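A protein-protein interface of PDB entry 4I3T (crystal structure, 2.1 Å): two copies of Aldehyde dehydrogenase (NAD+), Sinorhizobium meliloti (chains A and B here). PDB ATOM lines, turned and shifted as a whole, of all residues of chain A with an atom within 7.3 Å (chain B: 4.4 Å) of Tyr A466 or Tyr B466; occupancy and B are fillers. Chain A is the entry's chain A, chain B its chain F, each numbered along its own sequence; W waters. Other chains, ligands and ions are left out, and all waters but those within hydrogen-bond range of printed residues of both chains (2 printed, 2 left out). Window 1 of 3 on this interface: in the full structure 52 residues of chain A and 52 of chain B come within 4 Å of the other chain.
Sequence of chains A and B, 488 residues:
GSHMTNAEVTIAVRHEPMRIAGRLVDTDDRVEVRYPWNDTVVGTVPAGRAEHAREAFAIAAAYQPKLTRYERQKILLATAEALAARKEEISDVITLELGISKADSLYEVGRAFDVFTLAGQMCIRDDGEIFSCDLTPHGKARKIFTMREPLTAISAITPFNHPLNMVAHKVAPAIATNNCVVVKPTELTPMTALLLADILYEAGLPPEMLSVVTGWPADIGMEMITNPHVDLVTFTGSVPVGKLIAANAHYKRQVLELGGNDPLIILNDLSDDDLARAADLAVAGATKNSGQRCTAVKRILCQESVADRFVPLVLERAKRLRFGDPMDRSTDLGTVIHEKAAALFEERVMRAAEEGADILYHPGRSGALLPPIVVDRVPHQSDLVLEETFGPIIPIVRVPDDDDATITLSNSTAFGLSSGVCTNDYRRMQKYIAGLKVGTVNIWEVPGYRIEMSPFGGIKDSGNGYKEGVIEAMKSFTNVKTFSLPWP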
ATOM      1  N   LEU A 232      29.340  19.787  15.210  1.00  0.00           N
ATOM      2  CA  LEU A 232      28.291  19.273  14.345  1.00  0.00           C
ATOM      3  C   LEU A 232      27.516  18.162  15.046  1.00  0.00           C
ATOM      4  O   LEU A 232      28.111  17.274  15.654  1.00  0.00           O
ATOM      5  CB  LEU A 232      28.903  18.762  13.042  1.00  0.00           C
ATOM      6  CG  LEU A 232      27.928  18.209  11.987  1.00  0.00           C
ATOM      7  CD1 LEU A 232      28.438  18.515  10.589  1.00  0.00           C
ATOM      8  CD2 LEU A 232      27.690  16.706  12.151  1.00  0.00           C
ATOM      9  N   LYS A 252      25.622  25.491  15.847  1.00  0.00           N
ATOM     10  CA  LYS A 252      26.244  24.217  15.485  1.00  0.00           C
ATOM     11  C   LYS A 252      25.690  23.774  14.154  1.00  0.00           C
ATOM     12  O   LYS A 252      24.524  24.012  13.868  1.00  0.00           O
ATOM     13  CB  LYS A 252      25.905  23.135  16.514  1.00  0.00           C
ATOM     14  CG  LYS A 252      26.425  23.396  17.911  1.00  0.00           C
ATOM     15  CD  LYS A 252      26.110  22.223  18.841  1.00  0.00           C
ATOM     16  CE  LYS A 252      26.489  22.552  20.285  1.00  0.00           C
ATOM     17  NZ  LYS A 252      27.951  22.911  20.425  1.00  0.00           N
ATOM     18  N   ARG A 253      26.517  23.126  13.335  1.00  0.00           N
ATOM     19  CA  ARG A 253      25.992  22.526  12.122  1.00  0.00           C
ATOM     20  C   ARG A 253      25.093  21.371  12.534  1.00  0.00           C
ATOM     21  O   ARG A 253      25.362  20.679  13.530  1.00  0.00           O
ATOM     22  CB  ARG A 253      27.118  22.040  11.224  1.00  0.00           C
ATOM     23  CG  ARG A 253      28.279  22.974  11.211  1.00  0.00           C
ATOM     24  CD  ARG A 253      28.652  23.376   9.816  1.00  0.00           C
ATOM     25  NE  ARG A 253      29.605  22.463   9.191  1.00  0.00           N
ATOM     26  CZ  ARG A 253      30.926  22.494   9.373  1.00  0.00           C
ATOM     27  NH1 ARG A 253      31.484  23.376  10.202  1.00  0.00           N
ATOM     28  NH2 ARG A 253      31.697  21.624   8.732  1.00  0.00           N
ATOM     29  N   GLN A 254      24.009  21.191  11.793  1.00  0.00           N
ATOM     30  CA  GLN A 254      23.052  20.145  12.103  1.00  0.00           C
ATOM     31  C   GLN A 254      22.755  19.351  10.843  1.00  0.00           C
ATOM     32  O   GLN A 254      22.434  19.927   9.803  1.00  0.00           O
ATOM     33  CB  GLN A 254      21.765  20.755  12.633  1.00  0.00           C
ATOM     34  CG  GLN A 254      21.945  21.568  13.895  1.00  0.00           C
ATOM     35  CD  GLN A 254      20.808  22.555  14.112  1.00  0.00           C
ATOM     36  OE1 GLN A 254      19.676  22.340  13.671  1.00  0.00           O
ATOM     37  NE2 GLN A 254      21.114  23.651  14.774  1.00  0.00           N
ATOM     38  N   VAL A 255      22.888  18.035  10.926  1.00  0.00           N
ATOM     39  CA  VAL A 255      22.439  17.161   9.839  1.00  0.00           C
ATOM     40  C   VAL A 255      21.308  16.332  10.429  1.00  0.00           C
ATOM     41  O   VAL A 255      21.544  15.438  11.253  1.00  0.00           O
ATOM     42  CB  VAL A 255      23.577  16.269   9.325  1.00  0.00           C
ATOM     43  CG1 VAL A 255      23.091  15.358   8.193  1.00  0.00           C
ATOM     44  CG2 VAL A 255      24.763  17.136   8.870  1.00  0.00           C
ATOM     45  N   LEU A 256      20.079  16.662  10.044  1.00  0.00           N
ATOM     46  CA  LEU A 256      18.910  16.036  10.645  1.00  0.00           C
ATOM     47  C   LEU A 256      18.166  15.237   9.604  1.00  0.00           C
ATOM     48  O   LEU A 256      17.689  15.801   8.617  1.00  0.00           O
ATOM     49  CB  LEU A 256      17.978  17.092  11.229  1.00  0.00           C
ATOM     50  CG  LEU A 256      18.640  18.159  12.097  1.00  0.00           C
ATOM     51  CD1 LEU A 256      17.625  19.235  12.520  1.00  0.00           C
ATOM     52  CD2 LEU A 256      19.267  17.514  13.311  1.00  0.00           C
ATOM     53  N   GLU A 257      18.084  13.923   9.812  1.00  0.00           N
ATOM     54  CA  GLU A 257      17.278  13.079   8.941  1.00  0.00           C
ATOM     55  C   GLU A 257      16.119  12.568   9.771  1.00  0.00           C
ATOM     56  O   GLU A 257      16.316  11.922  10.790  1.00  0.00           O
ATOM     57  CB  GLU A 257      18.087  11.920   8.353  1.00  0.00           C
ATOM     58  CG  GLU A 257      19.369  12.331   7.642  1.00  0.00           C
ATOM     59  CD  GLU A 257      19.150  13.276   6.444  1.00  0.00           C
ATOM     60  OE1 GLU A 257      17.994  13.430   5.961  1.00  0.00           O
ATOM     61  OE2 GLU A 257      20.159  13.868   5.990  1.00  0.00           O
ATOM     62  N   PHE A 456      21.976  11.078   0.010  1.00  0.00           N
ATOM     63  CA  PHE A 456      20.742  10.660   0.659  1.00  0.00           C
ATOM     64  C   PHE A 456      20.254  11.710   1.633  1.00  0.00           C
ATOM     65  O   PHE A 456      21.008  12.137   2.508  1.00  0.00           O
ATOM     66  CB  PHE A 456      20.935   9.323   1.388  1.00  0.00           C
ATOM     67  CG  PHE A 456      19.763   8.924   2.248  1.00  0.00           C
ATOM     68  CD1 PHE A 456      18.569   8.491   1.669  1.00  0.00           C
ATOM     69  CD2 PHE A 456      19.845   8.985   3.628  1.00  0.00           C
ATOM     70  CE1 PHE A 456      17.472   8.125   2.452  1.00  0.00           C
ATOM     71  CE2 PHE A 456      18.755   8.624   4.426  1.00  0.00           C
ATOM     72  CZ  PHE A 456      17.562   8.191   3.829  1.00  0.00           C
ATOM     73  N   GLY A 457      18.993  12.115   1.491  1.00  0.00           N
ATOM     74  CA  GLY A 457      18.404  13.071   2.411  1.00  0.00           C
ATOM     75  C   GLY A 457      17.113  13.631   1.853  1.00  0.00           C
ATOM     76  O   GLY A 457      16.900  13.629   0.646  1.00  0.00           O
ATOM     77  N   GLY A 458      16.249  14.122   2.728  1.00  0.00           N
ATOM     78  CA  GLY A 458      14.951  14.587   2.287  1.00  0.00           C
ATOM     79  C   GLY A 458      14.728  16.069   2.500  1.00  0.00           C
ATOM     80  O   GLY A 458      15.623  16.817   2.887  1.00  0.00           O
ATOM     81  N   ILE A 459      13.504  16.497   2.243  1.00  0.00           N
ATOM     82  CA  ILE A 459      13.128  17.879   2.443  1.00  0.00           C
ATOM     83  C   ILE A 459      11.867  17.921   3.288  1.00  0.00           C
ATOM     84  O   ILE A 459      11.430  16.878   3.819  1.00  0.00           O
ATOM     85  CB  ILE A 459      12.907  18.569   1.086  1.00  0.00           C
ATOM     86  CG1 ILE A 459      11.843  17.826   0.273  1.00  0.00           C
ATOM     87  CG2 ILE A 459      14.197  18.617   0.326  1.00  0.00           C
ATOM     88  CD1 ILE A 459      11.556  18.474  -1.089  1.00  0.00           C
ATOM     89  N   GLY A 463      13.777  16.157   6.545  1.00  0.00           N
ATOM     90  CA  GLY A 463      15.155  16.527   6.811  1.00  0.00           C
ATOM     91  C   GLY A 463      15.403  18.003   6.607  1.00  0.00           C
ATOM     92  O   GLY A 463      14.652  18.661   5.870  1.00  0.00           O
ATOM     93  N   ASN A 464      16.446  18.527   7.259  1.00  0.00           N
ATOM     94  CA  ASN A 464      16.744  19.954   7.179  1.00  0.00           C
ATOM     95  C   ASN A 464      17.502  20.349   5.919  1.00  0.00           C
ATOM     96  O   ASN A 464      17.950  21.476   5.788  1.00  0.00           O
ATOM     97  CB  ASN A 464      17.425  20.486   8.450  1.00  0.00           C
ATOM     98  CG  ASN A 464      18.798  19.889   8.686  1.00  0.00           C
ATOM     99  OD1 ASN A 464      19.129  18.819   8.170  1.00  0.00           O
ATOM    100  ND2 ASN A 464      19.611  20.583   9.490  1.00  0.00           N
ATOM    101  N   GLY A 465      17.632  19.416   4.986  1.00  0.00           N
ATOM    102  CA  GLY A 465      18.106  19.762   3.661  1.00  0.00           C
ATOM    103  C   GLY A 465      19.570  19.466   3.374  1.00  0.00           C
ATOM    104  O   GLY A 465      20.094  19.866   2.343  1.00  0.00           O
ATOM    105  N   TYR A 466      20.240  18.771   4.279  1.00  0.00           N
ATOM    106  CA  TYR A 466      21.600  18.342   3.996  1.00  0.00           C
ATOM    107  C   TYR A 466      21.620  16.887   3.545  1.00  0.00           C
ATOM    108  O   TYR A 466      20.781  16.094   3.943  1.00  0.00           O
ATOM    109  CB  TYR A 466      22.500  18.576   5.205  1.00  0.00           C
ATOM    110  CG  TYR A 466      22.603  20.042   5.549  1.00  0.00           C
ATOM    111  CD1 TYR A 466      23.266  20.936   4.693  1.00  0.00           C
ATOM    112  CD2 TYR A 466      22.007  20.546   6.704  1.00  0.00           C
ATOM    113  CE1 TYR A 466      23.341  22.295   4.993  1.00  0.00           C
ATOM    114  CE2 TYR A 466      22.080  21.897   7.023  1.00  0.00           C
ATOM    115  CZ  TYR A 466      22.751  22.771   6.159  1.00  0.00           C
ATOM    116  OH  TYR A 466      22.836  24.116   6.448  1.00  0.00           O
ATOM    117  N   LYS A 467      22.562  16.540   2.686  1.00  0.00           N
ATOM    118  CA  LYS A 467      22.654  15.171   2.210  1.00  0.00           C
ATOM    119  C   LYS A 467      23.587  14.328   3.072  1.00  0.00           C
ATOM    120  O   LYS A 467      24.547  14.827   3.653  1.00  0.00           O
ATOM    121  CB  LYS A 467      23.098  15.128   0.748  1.00  0.00           C
ATOM    122  CG  LYS A 467      22.057  15.707  -0.199  1.00  0.00           C
ATOM    123  CD  LYS A 467      20.772  14.882  -0.196  1.00  0.00           C
ATOM    124  CE  LYS A 467      19.816  15.390  -1.274  1.00  0.00           C
ATOM    125  NZ  LYS A 467      18.644  14.489  -1.492  1.00  0.00           N
ATOM    126  N   GLU A 468      23.279  13.039   3.134  1.00  0.00           N
ATOM    127  CA  GLU A 468      24.041  12.067   3.898  1.00  0.00           C
ATOM    128  C   GLU A 468      24.517  11.026   2.879  1.00  0.00           C
ATOM    129  O   GLU A 468      24.445  11.240   1.669  1.00  0.00           O
ATOM    130  CB  GLU A 468      23.132  11.391   4.935  1.00  0.00           C
ATOM    131  CG  GLU A 468      23.539  11.531   6.386  1.00  0.00           C
ATOM    132  CD  GLU A 468      22.812  10.524   7.279  1.00  0.00           C
ATOM    133  OE1 GLU A 468      21.655  10.165   6.948  1.00  0.00           O
ATOM    134  OE2 GLU A 468      23.407  10.080   8.297  1.00  0.00           O
ATOM    135  N   GLU A 472      28.874  12.424   0.963  1.00  0.00           N
ATOM    136  CA  GLU A 472      28.375  13.707   1.450  1.00  0.00           C
ATOM    137  C   GLU A 472      28.657  13.892   2.932  1.00  0.00           C
ATOM    138  O   GLU A 472      28.900  15.006   3.392  1.00  0.00           O
ATOM    139  CB  GLU A 472      26.886  13.878   1.138  1.00  0.00           C
ATOM    140  CG  GLU A 472      26.599  14.011  -0.358  1.00  0.00           C
ATOM    141  CD  GLU A 472      27.238  15.259  -0.990  1.00  0.00           C
ATOM    142  OE1 GLU A 472      27.413  16.304  -0.301  1.00  0.00           O
ATOM    143  OE2 GLU A 472      27.586  15.180  -2.186  1.00  0.00           O
ATOM    144  N   SER A 476      30.484  16.898   4.859  1.00  0.00           N
ATOM    145  CA  SER A 476      29.839  17.561   6.003  1.00  0.00           C
ATOM    146  C   SER A 476      30.754  17.592   7.217  1.00  0.00           C
ATOM    147  O   SER A 476      30.692  18.511   8.027  1.00  0.00           O
ATOM    148  CB  SER A 476      28.544  16.832   6.398  1.00  0.00           C
ATOM    149  OG  SER A 476      27.516  17.063   5.451  1.00  0.00           O
ATOM    150  N   ASN A 479      35.901  21.053   7.357  1.00  0.00           N
ATOM    151  CA  ASN A 479      35.920  22.449   6.965  1.00  0.00           C
ATOM    152  C   ASN A 479      36.826  22.566   5.755  1.00  0.00           C
ATOM    153  O   ASN A 479      37.893  21.931   5.693  1.00  0.00           O
ATOM    154  CB  ASN A 479      36.489  23.321   8.094  1.00  0.00           C
ATOM    155  CG  ASN A 479      35.535  23.457   9.264  1.00  0.00           C
ATOM    156  OD1 ASN A 479      34.330  23.639   9.076  1.00  0.00           O
ATOM    157  ND2 ASN A 479      36.075  23.364  10.480  1.00  0.00           N
ATOM    158  N   ARG B 253      18.048  26.014   7.192  1.00  0.00           N
ATOM    159  CA  ARG B 253      19.463  26.082   6.865  1.00  0.00           C
ATOM    160  C   ARG B 253      19.924  27.500   7.150  1.00  0.00           C
ATOM    161  O   ARG B 253      19.186  28.446   6.959  1.00  0.00           O
ATOM    162  CB  ARG B 253      19.731  25.717   5.412  1.00  0.00           C
ATOM    163  CG  ARG B 253      18.831  24.601   4.923  1.00  0.00           C
ATOM    164  CD  ARG B 253      19.619  23.482   4.309  1.00  0.00           C
ATOM    165  NE  ARG B 253      19.852  23.686   2.884  1.00  0.00           N
ATOM    166  CZ  ARG B 253      18.977  23.406   1.919  1.00  0.00           C
ATOM    167  NH1 ARG B 253      17.755  22.919   2.192  1.00  0.00           N
ATOM    168  NH2 ARG B 253      19.329  23.628   0.665  1.00  0.00           N
ATOM    169  N   GLN B 254      21.154  27.615   7.634  1.00  0.00           N
ATOM    170  CA  GLN B 254      21.708  28.894   8.026  1.00  0.00           C
ATOM    171  C   GLN B 254      23.087  29.044   7.421  1.00  0.00           C
ATOM    172  O   GLN B 254      23.962  28.191   7.599  1.00  0.00           O
ATOM    173  CB  GLN B 254      21.822  28.976   9.550  1.00  0.00           C
ATOM    174  CG  GLN B 254      20.494  28.876  10.279  1.00  0.00           C
ATOM    175  CD  GLN B 254      20.671  28.457  11.726  1.00  0.00           C
ATOM    176  OE1 GLN B 254      21.683  28.772  12.358  1.00  0.00           O
ATOM    177  NE2 GLN B 254      19.696  27.721  12.250  1.00  0.00           N
ATOM    178  N   GLU B 257      27.870  34.457   8.134  1.00  0.00           N
ATOM    179  CA  GLU B 257      29.218  34.977   8.018  1.00  0.00           C
ATOM    180  C   GLU B 257      29.317  36.128   8.992  1.00  0.00           C
ATOM    181  O   GLU B 257      28.568  37.105   8.910  1.00  0.00           O
ATOM    182  CB  GLU B 257      29.548  35.424   6.587  1.00  0.00           C
ATOM    183  CG  GLU B 257      29.310  34.351   5.507  1.00  0.00           C
ATOM    184  CD  GLU B 257      30.131  33.059   5.702  1.00  0.00           C
ATOM    185  OE1 GLU B 257      31.084  33.037   6.532  1.00  0.00           O
ATOM    186  OE2 GLU B 257      29.810  32.062   5.005  1.00  0.00           O
ATOM    187  N   PHE B 456      34.366  30.980   0.055  1.00  0.00           N
ATOM    188  CA  PHE B 456      34.638  31.996   1.052  1.00  0.00           C
ATOM    189  C   PHE B 456      33.839  31.738   2.313  1.00  0.00           C
ATOM    190  O   PHE B 456      32.624  31.544   2.260  1.00  0.00           O
ATOM    191  CB  PHE B 456      34.297  33.387   0.514  1.00  0.00           C
ATOM    192  CG  PHE B 456      34.342  34.463   1.568  1.00  0.00           C
ATOM    193  CD1 PHE B 456      35.556  34.854   2.118  1.00  0.00           C
ATOM    194  CD2 PHE B 456      33.176  35.073   2.013  1.00  0.00           C
ATOM    195  CE1 PHE B 456      35.607  35.837   3.102  1.00  0.00           C
ATOM    196  CE2 PHE B 456      33.218  36.061   2.995  1.00  0.00           C
ATOM    197  CZ  PHE B 456      34.438  36.439   3.543  1.00  0.00           C
ATOM    198  N   GLY B 457      34.517  31.730   3.448  1.00  0.00           N
ATOM    199  CA  GLY B 457      33.831  31.544   4.716  1.00  0.00           C
ATOM    200  C   GLY B 457      34.802  31.177   5.808  1.00  0.00           C
ATOM    201  O   GLY B 457      35.873  30.630   5.534  1.00  0.00           O
ATOM    202  N   ASN B 464      29.543  29.836  10.764  1.00  0.00           N
ATOM    203  CA  ASN B 464      29.077  28.505  11.163  1.00  0.00           C
ATOM    204  C   ASN B 464      29.589  27.373  10.274  1.00  0.00           C
ATOM    205  O   ASN B 464      29.123  26.241  10.382  1.00  0.00           O
ATOM    206  CB  ASN B 464      27.549  28.451  11.323  1.00  0.00           C
ATOM    207  CG  ASN B 464      26.802  28.665  10.015  1.00  0.00           C
ATOM    208  OD1 ASN B 464      27.349  29.211   9.047  1.00  0.00           O
ATOM    209  ND2 ASN B 464      25.533  28.255   9.989  1.00  0.00           N
ATOM    210  N   GLY B 465      30.551  27.675   9.403  1.00  0.00           N
ATOM    211  CA  GLY B 465      31.233  26.638   8.642  1.00  0.00           C
ATOM    212  C   GLY B 465      30.739  26.314   7.234  1.00  0.00           C
ATOM    213  O   GLY B 465      31.184  25.343   6.627  1.00  0.00           O
ATOM    214  N   TYR B 466      29.820  27.110   6.705  1.00  0.00           N
ATOM    215  CA  TYR B 466      29.421  26.955   5.306  1.00  0.00           C
ATOM    216  C   TYR B 466      30.145  27.972   4.435  1.00  0.00           C
ATOM    217  O   TYR B 466      30.408  29.083   4.862  1.00  0.00           O
ATOM    218  CB  TYR B 466      27.900  27.072   5.150  1.00  0.00           C
ATOM    219  CG  TYR B 466      27.174  25.988   5.930  1.00  0.00           C
ATOM    220  CD1 TYR B 466      27.225  24.649   5.519  1.00  0.00           C
ATOM    221  CD2 TYR B 466      26.469  26.292   7.083  1.00  0.00           C
ATOM    222  CE1 TYR B 466      26.574  23.648   6.240  1.00  0.00           C
ATOM    223  CE2 TYR B 466      25.815  25.302   7.806  1.00  0.00           C
ATOM    224  CZ  TYR B 466      25.864  23.987   7.382  1.00  0.00           C
ATOM    225  OH  TYR B 466      25.207  23.025   8.120  1.00  0.00           O
ATOM    226  N   LYS B 467      30.479  27.575   3.216  1.00  0.00           N
ATOM    227  CA  LYS B 467      31.145  28.466   2.285  1.00  0.00           C
ATOM    228  C   LYS B 467      30.174  29.292   1.442  1.00  0.00           C
ATOM    229  O   LYS B 467      29.097  28.840   1.080  1.00  0.00           O
ATOM    230  CB  LYS B 467      32.087  27.683   1.373  1.00  0.00           C
ATOM    231  CG  LYS B 467      33.241  27.034   2.103  1.00  0.00           C
ATOM    232  CD  LYS B 467      34.168  28.106   2.701  1.00  0.00           C
ATOM    233  CE  LYS B 467      35.391  27.450   3.312  1.00  0.00           C
ATOM    234  NZ  LYS B 467      36.439  28.427   3.749  1.00  0.00           N
ATOM    235  N   GLU B 468      30.605  30.506   1.130  1.00  0.00           N
ATOM    236  CA  GLU B 468      29.873  31.450   0.302  1.00  0.00           C
ATOM    237  C   GLU B 468      30.719  31.679  -0.960  1.00  0.00           C
ATOM    238  O   GLU B 468      31.619  30.893  -1.266  1.00  0.00           O
ATOM    239  CB  GLU B 468      29.730  32.770   1.052  1.00  0.00           C
ATOM    240  CG  GLU B 468      28.312  33.212   1.352  1.00  0.00           C
ATOM    241  CD  GLU B 468      28.250  34.679   1.783  1.00  0.00           C
ATOM    242  OE1 GLU B 468      29.234  35.164   2.397  1.00  0.00           O
ATOM    243  OE2 GLU B 468      27.232  35.352   1.489  1.00  0.00           O
HETATM  244  O   HOH W   1      23.635  26.055   4.965  1.00  0.00           O
HETATM  245  O   HOH W   2      24.463  26.861  12.259  1.00  0.00           O
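Arg A253 touches Asn B464, and with the chains exchanged Asn A464 touches Arg B253.
Arg A253 touches Gly B465, and with the chains exchanged Gly A465 touches Arg B253.
Arg A253 touches Tyr B466, and with the chains exchanged Tyr A466 touches Arg B253.
Tyr B466 touches its own counterpart, Tyr A466.
10 positions are printed for both chains.
Of the 7 pairs that touch across the chains among the printed residues, 7 have their exchanged pair printed and touching as well.
OH of Tyr B466 is in hydrogen-bond range of OH of Tyr A466 (3.1 Å).
Among the printed residues, merely in contact across the chains: Arg A253 with Asn B464 (3.0 Å), Arg A253 with Gly B465 (3.6 Å), Arg A253 with Tyr B466 (3.8 Å), Asn A464 with Arg B253 (3.0 Å), Gly A465 with Arg B253 (3.5 Å) and Tyr A466 with Arg B253 (3.6 Å).
Water W1 bridges the side-chain hydroxyl of Tyr A466 and the backbone carbonyl oxygen of Gln B254.
Water W2 lies within hydrogen-bond range of ND2 of Asn B464 (2.9 Å), O of Lys A252 (3.3 Å) and OE1 of Gln B254 (3.4 Å).
Of the 10 printed residues of chain B, 4 touch a printed residue of chain A.
Along chain B the printed residues that touch a printed residue of chain A span positions 253 to 466.
Of the 20 printed residues of chain A, 4 touch a printed residue of chain B.
Among the printed residues, 7 pairs touch across the chains.
Among the printed residues, no Asp or Glu carboxylate lies within 4 Å of a Lys or Arg side-chain nitrogen of the other chain.
The backbone carbonyl oxygen (O) of Gln B254 lies within hydrogen-bond range of the side-chain amide nitrogen (ND2) of Asn B464 (2.9 Å).
The backbone carbonyl oxygen (O) of Gln A254 lies within hydrogen-bond range of the side-chain amide nitrogen (ND2) of Asn A464, at 2.9 Å.
The backbone carbonyl oxygen of Ser A476 is in hydrogen-bond range of the guanidinium group of Arg A253, 3.3 Å away.
The backbone NH (N) of Leu A256 lies within hydrogen-bond range of the side-chain amide oxygen (OD1) of Asn A464 (3.0 Å).
NH1 of Arg A253 sits at hydrogen-bond distance from OD1 of Asn A479, at 3.1 Å.
Printed residues of chain A within 4 Å of Tyr B466: Arg A253 and Tyr A466.
Gly B465 touches just one residue of chain A: Arg A253.
Of the printed residues of chain B, Arg A253 touches Asn B464, Gly B465 and Tyr B466.
Printed residues of chain A within 4 Å of Arg B253: Asn A464, Gly A465 and Tyr A466.
Of the printed residues of chain A, Asn B464 touches Arg A253.
Printed residues of chain B within 4 Å of Asn A464: Arg B253.
Printed residues of chain B within 4 Å of Gly A465: Arg B253.
Gly A458 touches none of the printed residues of chain B.
Lys B467 touches none of the printed residues of chain A.
The nearest residue of chain A that does not touch Tyr B466 is Gln A254 (4.3 Å).
The nearest printed residue of chain B that does not touch Asn A464 is Tyr B466 (6.3 Å).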
